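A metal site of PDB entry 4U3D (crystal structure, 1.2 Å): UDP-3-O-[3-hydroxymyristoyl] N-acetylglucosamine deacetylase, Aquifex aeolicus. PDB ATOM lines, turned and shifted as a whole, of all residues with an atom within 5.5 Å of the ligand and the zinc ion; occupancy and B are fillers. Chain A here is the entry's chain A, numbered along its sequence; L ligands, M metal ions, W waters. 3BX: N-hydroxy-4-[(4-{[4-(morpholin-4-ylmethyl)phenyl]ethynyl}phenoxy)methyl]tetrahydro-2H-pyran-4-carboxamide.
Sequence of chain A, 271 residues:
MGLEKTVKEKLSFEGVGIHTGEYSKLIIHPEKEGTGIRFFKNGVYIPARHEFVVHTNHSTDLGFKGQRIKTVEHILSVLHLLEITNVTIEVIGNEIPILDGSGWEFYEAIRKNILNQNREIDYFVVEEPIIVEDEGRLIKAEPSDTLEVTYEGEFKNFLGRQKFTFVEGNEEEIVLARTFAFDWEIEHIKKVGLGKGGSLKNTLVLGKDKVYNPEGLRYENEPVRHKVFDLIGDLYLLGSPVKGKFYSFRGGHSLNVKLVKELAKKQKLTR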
ATOM      1  N   ILE A  18       3.902 -32.853   1.154  1.00  0.00           N
ATOM      2  CA  ILE A  18       4.723 -32.313   0.066  1.00  0.00           C
ATOM      3  C   ILE A  18       5.791 -33.279  -0.414  1.00  0.00           C
ATOM      4  O   ILE A  18       6.095 -33.286  -1.606  1.00  0.00           O
ATOM      5  CB  ILE A  18       5.314 -30.945   0.433  1.00  0.00           C
ATOM      6  CG1 ILE A  18       5.654 -30.174  -0.881  1.00  0.00           C
ATOM      7  CG2 ILE A  18       6.497 -31.034   1.400  1.00  0.00           C
ATOM      8  CD1 ILE A  18       5.946 -28.756  -0.706  1.00  0.00           C
ATOM      9  N   HIS A  19       6.383 -34.051   0.487  1.00  0.00           N
ATOM     10  CA  HIS A  19       7.473 -34.944   0.074  1.00  0.00           C
ATOM     11  C   HIS A  19       7.019 -36.337  -0.295  1.00  0.00           C
ATOM     12  O   HIS A  19       7.515 -36.902  -1.286  1.00  0.00           O
ATOM     13  CB  HIS A  19       8.568 -34.990   1.123  1.00  0.00           C
ATOM     14  CG  HIS A  19       9.337 -33.718   1.163  1.00  0.00           C
ATOM     15  ND1 HIS A  19       9.901 -33.183   0.007  1.00  0.00           N
ATOM     16  CD2 HIS A  19       9.651 -32.911   2.209  1.00  0.00           C
ATOM     17  CE1 HIS A  19      10.509 -32.063   0.367  1.00  0.00           C
ATOM     18  NE2 HIS A  19      10.367 -31.845   1.686  1.00  0.00           N
ATOM     19  N   HIS A  58      15.706 -30.945   3.248  1.00  0.00           N
ATOM     20  CA  HIS A  58      14.500 -30.477   2.581  1.00  0.00           C
ATOM     21  C   HIS A  58      13.261 -30.490   3.460  1.00  0.00           C
ATOM     22  O   HIS A  58      12.204 -30.106   2.981  1.00  0.00           O
ATOM     23  CB  HIS A  58      14.227 -31.181   1.223  1.00  0.00           C
ATOM     24  CG  HIS A  58      15.428 -31.192   0.313  1.00  0.00           C
ATOM     25  ND1 HIS A  58      15.846 -30.054  -0.337  1.00  0.00           N
ATOM     26  CD2 HIS A  58      16.318 -32.189   0.075  1.00  0.00           C
ATOM     27  CE1 HIS A  58      16.984 -30.394  -0.966  1.00  0.00           C
ATOM     28  NE2 HIS A  58      17.271 -31.683  -0.800  1.00  0.00           N
ATOM     29  N   SER A  59      13.380 -30.931   4.730  1.00  0.00           N
ATOM     30  CA  SER A  59      12.321 -30.865   5.743  1.00  0.00           C
ATOM     31  C   SER A  59      12.958 -31.301   7.036  1.00  0.00           C
ATOM     32  O   SER A  59      14.067 -31.829   7.046  1.00  0.00           O
ATOM     33  CB  SER A  59      11.129 -31.760   5.397  1.00  0.00           C
ATOM     34  OG  SER A  59      11.516 -33.130   5.287  1.00  0.00           O
ATOM     35  N   THR A  71       8.273 -33.672   7.868  1.00  0.00           N
ATOM     36  CA  THR A  71       7.852 -32.297   7.640  1.00  0.00           C
ATOM     37  C   THR A  71       7.063 -31.728   8.788  1.00  0.00           C
ATOM     38  O   THR A  71       5.915 -31.269   8.619  1.00  0.00           O
ATOM     39  CB  THR A  71       7.127 -32.154   6.275  1.00  0.00           C
ATOM     40  OG1 THR A  71       7.806 -32.976   5.292  1.00  0.00           O
ATOM     41  CG2 THR A  71       7.082 -30.694   5.793  1.00  0.00           C
ATOM     42  N   GLU A  73       7.968 -29.019  10.553  1.00  0.00           N
ATOM     43  CA  GLU A  73       8.305 -27.631  10.852  1.00  0.00           C
ATOM     44  C   GLU A  73       7.175 -26.621  10.756  1.00  0.00           C
ATOM     45  O   GLU A  73       7.183 -25.653  11.518  1.00  0.00           O
ATOM     46  CB  GLU A  73       9.488 -27.160   9.977  1.00  0.00           C
ATOM     47  CG  GLU A  73       9.265 -27.287   8.481  1.00  0.00           C
ATOM     48  CD  GLU A  73       9.697 -28.591   7.810  1.00  0.00           C
ATOM     49  OE1 GLU A  73       9.783 -29.637   8.483  1.00  0.00           O
ATOM     50  OE2 GLU A  73       9.954 -28.570   6.588  1.00  0.00           O
ATOM     51  N   HIS A  74       6.197 -26.828   9.887  1.00  0.00           N
ATOM     52  CA  HIS A  74       5.110 -25.839   9.736  1.00  0.00           C
ATOM     53  C   HIS A  74       4.135 -25.901  10.867  1.00  0.00           C
ATOM     54  O   HIS A  74       3.766 -24.862  11.433  1.00  0.00           O
ATOM     55  CB  HIS A  74       4.377 -25.943   8.387  1.00  0.00           C
ATOM     56  CG  HIS A  74       5.246 -25.698   7.182  1.00  0.00           C
ATOM     57  ND1 HIS A  74       4.771 -25.844   5.880  1.00  0.00           N
ATOM     58  CD2 HIS A  74       6.545 -25.324   7.120  1.00  0.00           C
ATOM     59  CE1 HIS A  74       5.798 -25.591   5.083  1.00  0.00           C
ATOM     60  NE2 HIS A  74       6.881 -25.284   5.782  1.00  0.00           N
ATOM     61  N   THR A 179       5.887 -22.350   1.296  1.00  0.00           N
ATOM     62  CA  THR A 179       7.068 -23.089   0.907  1.00  0.00           C
ATOM     63  C   THR A 179       7.354 -22.762  -0.598  1.00  0.00           C
ATOM     64  O   THR A 179       6.428 -22.419  -1.349  1.00  0.00           O
ATOM     65  CB  THR A 179       6.854 -24.575   1.150  1.00  0.00           C
ATOM     66  OG1 THR A 179       8.109 -25.219   1.078  1.00  0.00           O
ATOM     67  CG2 THR A 179       5.861 -25.205   0.228  1.00  0.00           C
ATOM     68  N   PHE A 180       8.601 -22.895  -0.992  1.00  0.00           N
ATOM     69  CA  PHE A 180       9.009 -22.499  -2.334  1.00  0.00           C
ATOM     70  C   PHE A 180      10.094 -23.397  -2.825  1.00  0.00           C
ATOM     71  O   PHE A 180      10.795 -24.051  -2.037  1.00  0.00           O
ATOM     72  CB  PHE A 180       9.471 -21.018  -2.323  1.00  0.00           C
ATOM     73  CG  PHE A 180      10.664 -20.742  -1.452  1.00  0.00           C
ATOM     74  CD1 PHE A 180      11.944 -20.698  -1.987  1.00  0.00           C
ATOM     75  CD2 PHE A 180      10.513 -20.537  -0.088  1.00  0.00           C
ATOM     76  CE1 PHE A 180      13.055 -20.505  -1.170  1.00  0.00           C
ATOM     77  CE2 PHE A 180      11.626 -20.303   0.728  1.00  0.00           C
ATOM     78  CZ  PHE A 180      12.876 -20.287   0.183  1.00  0.00           C
ATOM     79  N   ALA A 181      10.293 -23.402  -4.153  1.00  0.00           N
ATOM     80  CA  ALA A 181      11.303 -24.217  -4.806  1.00  0.00           C
ATOM     81  C   ALA A 181      11.756 -23.511  -6.070  1.00  0.00           C
ATOM     82  O   ALA A 181      11.002 -22.751  -6.681  1.00  0.00           O
ATOM     83  CB  ALA A 181      10.730 -25.589  -5.175  1.00  0.00           C
ATOM     84  N   ILE A 186      14.437 -28.877  -8.842  1.00  0.00           N
ATOM     85  CA  ILE A 186      13.353 -29.866  -8.738  1.00  0.00           C
ATOM     86  C   ILE A 186      13.818 -31.261  -9.185  1.00  0.00           C
ATOM     87  O   ILE A 186      13.480 -32.246  -8.503  1.00  0.00           O
ATOM     88  CB  ILE A 186      12.067 -29.352  -9.453  1.00  0.00           C
ATOM     89  CG1 ILE A 186      11.472 -28.164  -8.633  1.00  0.00           C
ATOM     90  CG2 ILE A 186      11.022 -30.484  -9.588  1.00  0.00           C
ATOM     91  CD1 ILE A 186      10.303 -27.416  -9.285  1.00  0.00           C
ATOM     92  N   ILE A 189      15.502 -32.893  -6.146  1.00  0.00           N
ATOM     93  CA  ILE A 189      14.577 -33.274  -5.090  1.00  0.00           C
ATOM     94  C   ILE A 189      13.743 -34.527  -5.492  1.00  0.00           C
ATOM     95  O   ILE A 189      13.512 -35.416  -4.660  1.00  0.00           O
ATOM     96  CB  ILE A 189      13.742 -32.025  -4.689  1.00  0.00           C
ATOM     97  CG1 ILE A 189      14.676 -30.902  -4.184  1.00  0.00           C
ATOM     98  CG2 ILE A 189      12.702 -32.388  -3.626  1.00  0.00           C
ATOM     99  CD1 ILE A 189      14.006 -29.537  -4.012  1.00  0.00           C
ATOM    100  N   LYS A 190      13.371 -34.646  -6.771  1.00  0.00           N
ATOM    101  CA  LYS A 190      12.674 -35.831  -7.226  1.00  0.00           C
ATOM    102  C   LYS A 190      13.604 -37.052  -7.225  1.00  0.00           C
ATOM    103  O   LYS A 190      13.165 -38.126  -6.800  1.00  0.00           O
ATOM    104  CB  LYS A 190      12.082 -35.596  -8.608  1.00  0.00           C
ATOM    105  CG  LYS A 190      11.051 -34.466  -8.667  1.00  0.00           C
ATOM    106  CD  LYS A 190       9.848 -34.683  -7.763  1.00  0.00           C
ATOM    107  CE  LYS A 190       8.664 -34.002  -8.378  1.00  0.00           C
ATOM    108  NZ  LYS A 190       7.668 -34.988  -8.876  1.00  0.00           N
ATOM    109  N   GLY A 195       9.695 -34.415  -2.660  1.00  0.00           N
ATOM    110  CA  GLY A 195       8.862 -33.513  -3.461  1.00  0.00           C
ATOM    111  C   GLY A 195       7.736 -34.159  -4.231  1.00  0.00           C
ATOM    112  O   GLY A 195       7.169 -33.512  -5.127  1.00  0.00           O
ATOM    113  N   GLY A 198       4.581 -32.041  -4.307  1.00  0.00           N
ATOM    114  CA  GLY A 198       4.742 -30.649  -4.685  1.00  0.00           C
ATOM    115  C   GLY A 198       4.005 -30.310  -5.965  1.00  0.00           C
ATOM    116  O   GLY A 198       4.044 -31.069  -6.962  1.00  0.00           O
ATOM    117  N   SER A 199       3.305 -29.193  -5.957  1.00  0.00           N
ATOM    118  CA  SER A 199       2.599 -28.716  -7.142  1.00  0.00           C
ATOM    119  C   SER A 199       2.482 -27.192  -7.045  1.00  0.00           C
ATOM    120  O   SER A 199       2.755 -26.613  -5.986  1.00  0.00           O
ATOM    121  CB  SER A 199       1.202 -29.325  -7.237  1.00  0.00           C
ATOM    122  OG  SER A 199       0.336 -28.707  -6.309  1.00  0.00           O
ATOM    123  N   LEU A 200       1.937 -26.558  -8.080  1.00  0.00           N
ATOM    124  CA  LEU A 200       1.715 -25.120  -8.034  1.00  0.00           C
ATOM    125  C   LEU A 200       0.571 -24.791  -7.098  1.00  0.00           C
ATOM    126  O   LEU A 200       0.376 -23.604  -6.790  1.00  0.00           O
ATOM    127  CB  LEU A 200       1.511 -24.538  -9.445  1.00  0.00           C
ATOM    128  CG  LEU A 200       2.716 -24.700 -10.382  1.00  0.00           C
ATOM    129  CD1 LEU A 200       2.432 -24.061 -11.755  1.00  0.00           C
ATOM    130  CD2 LEU A 200       3.971 -24.054  -9.807  1.00  0.00           C
ATOM    131  N   ASN A 202       0.530 -25.866  -3.930  1.00  0.00           N
ATOM    132  CA  ASN A 202       1.054 -25.789  -2.555  1.00  0.00           C
ATOM    133  C   ASN A 202       2.476 -25.264  -2.470  1.00  0.00           C
ATOM    134  O   ASN A 202       3.005 -25.183  -1.359  1.00  0.00           O
ATOM    135  CB  ASN A 202       0.949 -27.170  -1.878  1.00  0.00           C
ATOM    136  CG  ASN A 202       1.642 -28.256  -2.675  1.00  0.00           C
ATOM    137  OD1 ASN A 202       2.693 -28.101  -3.275  1.00  0.00           O
ATOM    138  ND2 ASN A 202       1.021 -29.446  -2.691  1.00  0.00           N
ATOM    139  N   THR A 203       3.110 -24.881  -3.590  1.00  0.00           N
ATOM    140  CA  THR A 203       4.480 -24.415  -3.597  1.00  0.00           C
ATOM    141  C   THR A 203       4.610 -23.220  -4.519  1.00  0.00           C
ATOM    142  O   THR A 203       4.068 -23.244  -5.635  1.00  0.00           O
ATOM    143  CB  THR A 203       5.424 -25.522  -4.154  1.00  0.00           C
ATOM    144  OG1 THR A 203       5.231 -26.731  -3.389  1.00  0.00           O
ATOM    145  CG2 THR A 203       6.873 -25.173  -4.106  1.00  0.00           C
ATOM    146  N   VAL A 205       6.842 -21.745  -7.068  1.00  0.00           N
ATOM    147  CA  VAL A 205       7.951 -22.209  -7.892  1.00  0.00           C
ATOM    148  C   VAL A 205       8.495 -21.067  -8.728  1.00  0.00           C
ATOM    149  O   VAL A 205       7.723 -20.402  -9.443  1.00  0.00           O
ATOM    150  CB  VAL A 205       7.547 -23.419  -8.767  1.00  0.00           C
ATOM    151  CG1 VAL A 205       8.736 -23.894  -9.594  1.00  0.00           C
ATOM    152  CG2 VAL A 205       7.051 -24.560  -7.880  1.00  0.00           C
ATOM    153  N   TYR A 212       6.342 -19.239 -11.740  1.00  0.00           N
ATOM    154  CA  TYR A 212       5.441 -20.197 -12.378  1.00  0.00           C
ATOM    155  C   TYR A 212       4.001 -20.025 -11.981  1.00  0.00           C
ATOM    156  O   TYR A 212       3.093 -20.239 -12.795  1.00  0.00           O
ATOM    157  CB  TYR A 212       5.897 -21.626 -12.068  1.00  0.00           C
ATOM    158  CG  TYR A 212       7.080 -22.090 -12.865  1.00  0.00           C
ATOM    159  CD1 TYR A 212       8.366 -21.641 -12.563  1.00  0.00           C
ATOM    160  CD2 TYR A 212       6.944 -23.058 -13.854  1.00  0.00           C
ATOM    161  CE1 TYR A 212       9.482 -22.100 -13.281  1.00  0.00           C
ATOM    162  CE2 TYR A 212       8.039 -23.484 -14.605  1.00  0.00           C
ATOM    163  CZ  TYR A 212       9.308 -23.032 -14.301  1.00  0.00           C
ATOM    164  OH  TYR A 212      10.390 -23.508 -14.986  1.00  0.00           O
ATOM    165  N   HIS A 226       8.968 -17.144   4.567  1.00  0.00           N
ATOM    166  CA  HIS A 226       8.796 -18.559   4.797  1.00  0.00           C
ATOM    167  C   HIS A 226       9.990 -19.135   5.530  1.00  0.00           C
ATOM    168  O   HIS A 226       9.796 -19.983   6.408  1.00  0.00           O
ATOM    169  CB  HIS A 226       8.525 -19.316   3.488  1.00  0.00           C
ATOM    170  CG  HIS A 226       8.175 -20.742   3.776  1.00  0.00           C
ATOM    171  ND1 HIS A 226       6.916 -21.097   4.189  1.00  0.00           N
ATOM    172  CD2 HIS A 226       8.981 -21.839   3.877  1.00  0.00           C
ATOM    173  CE1 HIS A 226       6.963 -22.397   4.484  1.00  0.00           C
ATOM    174  NE2 HIS A 226       8.175 -22.894   4.318  1.00  0.00           N
ATOM    175  N   LYS A 227      11.199 -18.719   5.194  1.00  0.00           N
ATOM    176  CA  LYS A 227      12.378 -19.227   5.901  1.00  0.00           C
ATOM    177  C   LYS A 227      12.371 -18.826   7.366  1.00  0.00           C
ATOM    178  O   LYS A 227      12.817 -19.614   8.215  1.00  0.00           O
ATOM    179  CB  LYS A 227      13.664 -18.765   5.206  1.00  0.00           C
ATOM    180  CG  LYS A 227      13.825 -19.412   3.829  1.00  0.00           C
ATOM    181  CD  LYS A 227      14.063 -20.913   3.860  1.00  0.00           C
ATOM    182  CE  LYS A 227      15.491 -21.264   4.079  1.00  0.00           C
ATOM    183  NZ  LYS A 227      15.764 -22.726   3.813  1.00  0.00           N
ATOM    184  N   PHE A 229       9.599 -18.435   9.121  1.00  0.00           N
ATOM    185  CA  PHE A 229       8.564 -19.352   9.611  1.00  0.00           C
ATOM    186  C   PHE A 229       9.159 -20.758   9.861  1.00  0.00           C
ATOM    187  O   PHE A 229       8.931 -21.345  10.940  1.00  0.00           O
ATOM    188  CB  PHE A 229       7.413 -19.344   8.598  1.00  0.00           C
ATOM    189  CG  PHE A 229       6.287 -20.308   8.899  1.00  0.00           C
ATOM    190  CD1 PHE A 229       5.367 -20.015   9.886  1.00  0.00           C
ATOM    191  CD2 PHE A 229       6.142 -21.473   8.184  1.00  0.00           C
ATOM    192  CE1 PHE A 229       4.302 -20.887  10.158  1.00  0.00           C
ATOM    193  CE2 PHE A 229       5.054 -22.325   8.430  1.00  0.00           C
ATOM    194  CZ  PHE A 229       4.165 -22.033   9.434  1.00  0.00           C
ATOM    195  N   ASP A 230       9.968 -21.274   8.938  1.00  0.00           N
ATOM    196  CA  ASP A 230      10.605 -22.585   9.147  1.00  0.00           C
ATOM    197  C   ASP A 230      11.508 -22.570  10.368  1.00  0.00           C
ATOM    198  O   ASP A 230      11.510 -23.544  11.158  1.00  0.00           O
ATOM    199  CB  ASP A 230      11.470 -22.925   7.925  1.00  0.00           C
ATOM    200  CG  ASP A 230      10.742 -23.433   6.706  1.00  0.00           C
ATOM    201  OD1 ASP A 230       9.576 -23.846   6.852  1.00  0.00           O
ATOM    202  OD2 ASP A 230      11.370 -23.485   5.625  1.00  0.00           O
ATOM    203  N   HIS A 253      17.247 -26.296   7.353  1.00  0.00           N
ATOM    204  CA  HIS A 253      16.932 -27.143   8.508  1.00  0.00           C
ATOM    205  C   HIS A 253      18.131 -27.758   9.192  1.00  0.00           C
ATOM    206  O   HIS A 253      18.173 -27.843  10.405  1.00  0.00           O
ATOM    207  CB  HIS A 253      15.944 -28.246   8.160  1.00  0.00           C
ATOM    208  CG  HIS A 253      14.720 -27.728   7.515  1.00  0.00           C
ATOM    209  ND1 HIS A 253      13.798 -26.941   8.207  1.00  0.00           N
ATOM    210  CD2 HIS A 253      14.283 -27.880   6.238  1.00  0.00           C
ATOM    211  CE1 HIS A 253      12.841 -26.653   7.333  1.00  0.00           C
ATOM    212  NE2 HIS A 253      13.094 -27.183   6.137  1.00  0.00           N
HETATM  213  C1  3BX L   1       7.045 -29.947  -8.969  1.00  0.00           C
HETATM  214  C2  3BX L   1       7.742 -29.941  -7.772  1.00  0.00           C
HETATM  215  C3  3BX L   1       7.447 -28.982  -6.809  1.00  0.00           C
HETATM  216  C7  3BX L   1       5.301 -28.957 -10.485  1.00  0.00           C
HETATM  217  C9  3BX L   1       6.465 -27.056 -11.439  1.00  0.00           C
HETATM  218  C10 3BX L   1       7.253 -26.630 -12.664  1.00  0.00           C
HETATM  219  C12 3BX L   1       5.924 -28.020 -14.016  1.00  0.00           C
HETATM  220  C13 3BX L   1       5.140 -28.509 -12.798  1.00  0.00           C
HETATM  221  C14 3BX L   1       8.116 -28.928  -5.566  1.00  0.00           C
HETATM  222  C15 3BX L   1       8.656 -28.792  -4.500  1.00  0.00           C
HETATM  223  C16 3BX L   1       9.295 -28.562  -3.248  1.00  0.00           C
HETATM  224  C19 3BX L   1      10.596 -28.154  -0.853  1.00  0.00           C
HETATM  225  C20 3BX L   1      11.208 -28.881  -1.856  1.00  0.00           C
HETATM  226  C21 3BX L   1      10.535 -29.082  -3.040  1.00  0.00           C
HETATM  227  C24 3BX L   1      11.424 -26.313   2.104  1.00  0.00           C
HETATM  228  C30 3BX L   1      10.601 -25.985   3.343  1.00  0.00           C
HETATM  229  C4  3BX L   1       6.489 -28.036  -7.047  1.00  0.00           C
HETATM  230  C17 3BX L   1       8.700 -27.796  -2.261  1.00  0.00           C
HETATM  231  C5  3BX L   1       5.810 -28.034  -8.253  1.00  0.00           C
HETATM  232  C18 3BX L   1       9.352 -27.598  -1.046  1.00  0.00           C
HETATM  233  C6  3BX L   1       6.077 -28.992  -9.205  1.00  0.00           C
HETATM  234  C25 3BX L   1      12.872 -26.681   2.463  1.00  0.00           C
HETATM  235  C29 3BX L   1      11.482 -25.123   1.134  1.00  0.00           C
HETATM  236  C26 3BX L   1      13.635 -25.481   2.996  1.00  0.00           C
HETATM  237  C28 3BX L   1      12.318 -23.988   1.737  1.00  0.00           C
HETATM  238  C23 3BX L   1      10.682 -27.491   1.462  1.00  0.00           C
HETATM  239  N8  3BX L   1       6.039 -28.441 -11.641  1.00  0.00           N
HETATM  240  N32 3BX L   1      11.009 -26.624   4.479  1.00  0.00           N
HETATM  241  O31 3BX L   1       9.591 -25.277   3.291  1.00  0.00           O
HETATM  242  O27 3BX L   1      13.653 -24.437   2.025  1.00  0.00           O
HETATM  243  O11 3BX L   1       6.368 -26.679 -13.788  1.00  0.00           O
HETATM  244  O33 3BX L   1      10.142 -26.359   5.553  1.00  0.00           O
HETATM  245  O22 3BX L   1      11.381 -27.957   0.289  1.00  0.00           O
HETATM  246 ZN    ZN M   1       8.871 -24.659   5.127  1.00  0.00          ZN
HETATM  247  O   HOH W   1       8.147 -30.368 -12.449  1.00  0.00           O
HETATM  248  O   HOH W   2       6.034 -32.941  -7.514  1.00  0.00           O
HETATM  249  O   HOH W   3      16.035 -25.623   4.711  1.00  0.00           O
HETATM  250  O   HOH W   4      15.178 -23.586  -0.612  1.00  0.00           O
HETATM  251  O   HOH W   5       4.119 -25.265 -14.910  1.00  0.00           O
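NZ of Lys 227 is in hydrogen-bond range of O27 of the ligand.
The side-chain hydroxyl (OG1) of Thr 179 lies close to an oxygen (O31) of the ligand (2.7 Å).
The side-chain carboxylate (OE2) of Glu 73 lies within hydrogen-bond range of a nitrogen (N32) of the ligand, 3.1 Å away.
A nitrogen (N32) of the ligand is in hydrogen-bond range of a ring nitrogen (NE2) of His 253.
Along chain A the residues within 4 Å of the zinc ion span positions 74 to 230.
The backbone NH of Ser 199 is in hydrogen-bond range of the side-chain amide oxygen of Asn 202, at 3.0 Å.
A ring nitrogen (NE2) of His 19 lies within hydrogen-bond range of the backbone carbonyl oxygen (O) of His 58 (2.8 Å).
A ring nitrogen (ND1) of His 226 is in hydrogen-bond range of the backbone NH (N) of Thr 179, 3.3 Å away.
The backbone NH (N) of Gly 198 sits at hydrogen-bond distance from the backbone carbonyl oxygen (O) of Ile 18, 3.3 Å away.
A ring nitrogen (ND1) of His 19 sits at hydrogen-bond distance from the backbone NH (N) of Gly 195 (2.9 Å).
The side-chain hydroxyl (OG1) of Thr 203 sits at hydrogen-bond distance from the side-chain amide oxygen (OD1) of Asn 202.
N of Tyr 212 lies within hydrogen-bond range of O of Val 205.
The side-chain carboxylate (OE2) of Glu 73 sits at hydrogen-bond distance from a ring nitrogen (NE2) of His 253, 3.5 Å away.
The zinc ion is bound by OD1 of Asp 230, NE2 of His 226, O31 of the ligand, O33 of the ligand and NE2 of His 74.
Slightly farther from the zinc ion lies OD2 of Asp 230 (2.8 Å).
CD1 of Ile 18 touches C17 of the ligand, at 3.3 Å.
His 19 touches the ligand (CE1 to C20, 3.9 Å).
O of His 58 touches C23 of the ligand, at 3.4 Å.
Phe 180 touches the ligand.
Ala 181 touches the ligand.
Ile 186 touches the ligand (CG2 to C2, 3.8 Å).
CD1 of Ile 189 touches C20 of the ligand (3.6 Å).
C of Gly 198 touches C4 of the ligand (3.5 Å).
CA of Ser 199 touches C5 of the ligand, at 3.5 Å.
Thr 203 touches the ligand.
Val 205 touches the ligand (CG2 to C4, 3.6 Å).
Tyr 212 touches the ligand (CD2 to O11, 3.7 Å).
Hydrophobic or aromatic side chains within 4 Å of the ligand: Ile 18, His 19, Phe 180, Ala 181, Ile 186, Ile 189, Val 205, Tyr 212, His 226 and His 253.
Water W3 lies within hydrogen-bond range of N of His 253 (3.0 Å) and NZ of Lys 227 (3.0 Å).
Water W2 lies within hydrogen-bond range of O of Gly 195, O of Gly 198 and NZ of Lys 190.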
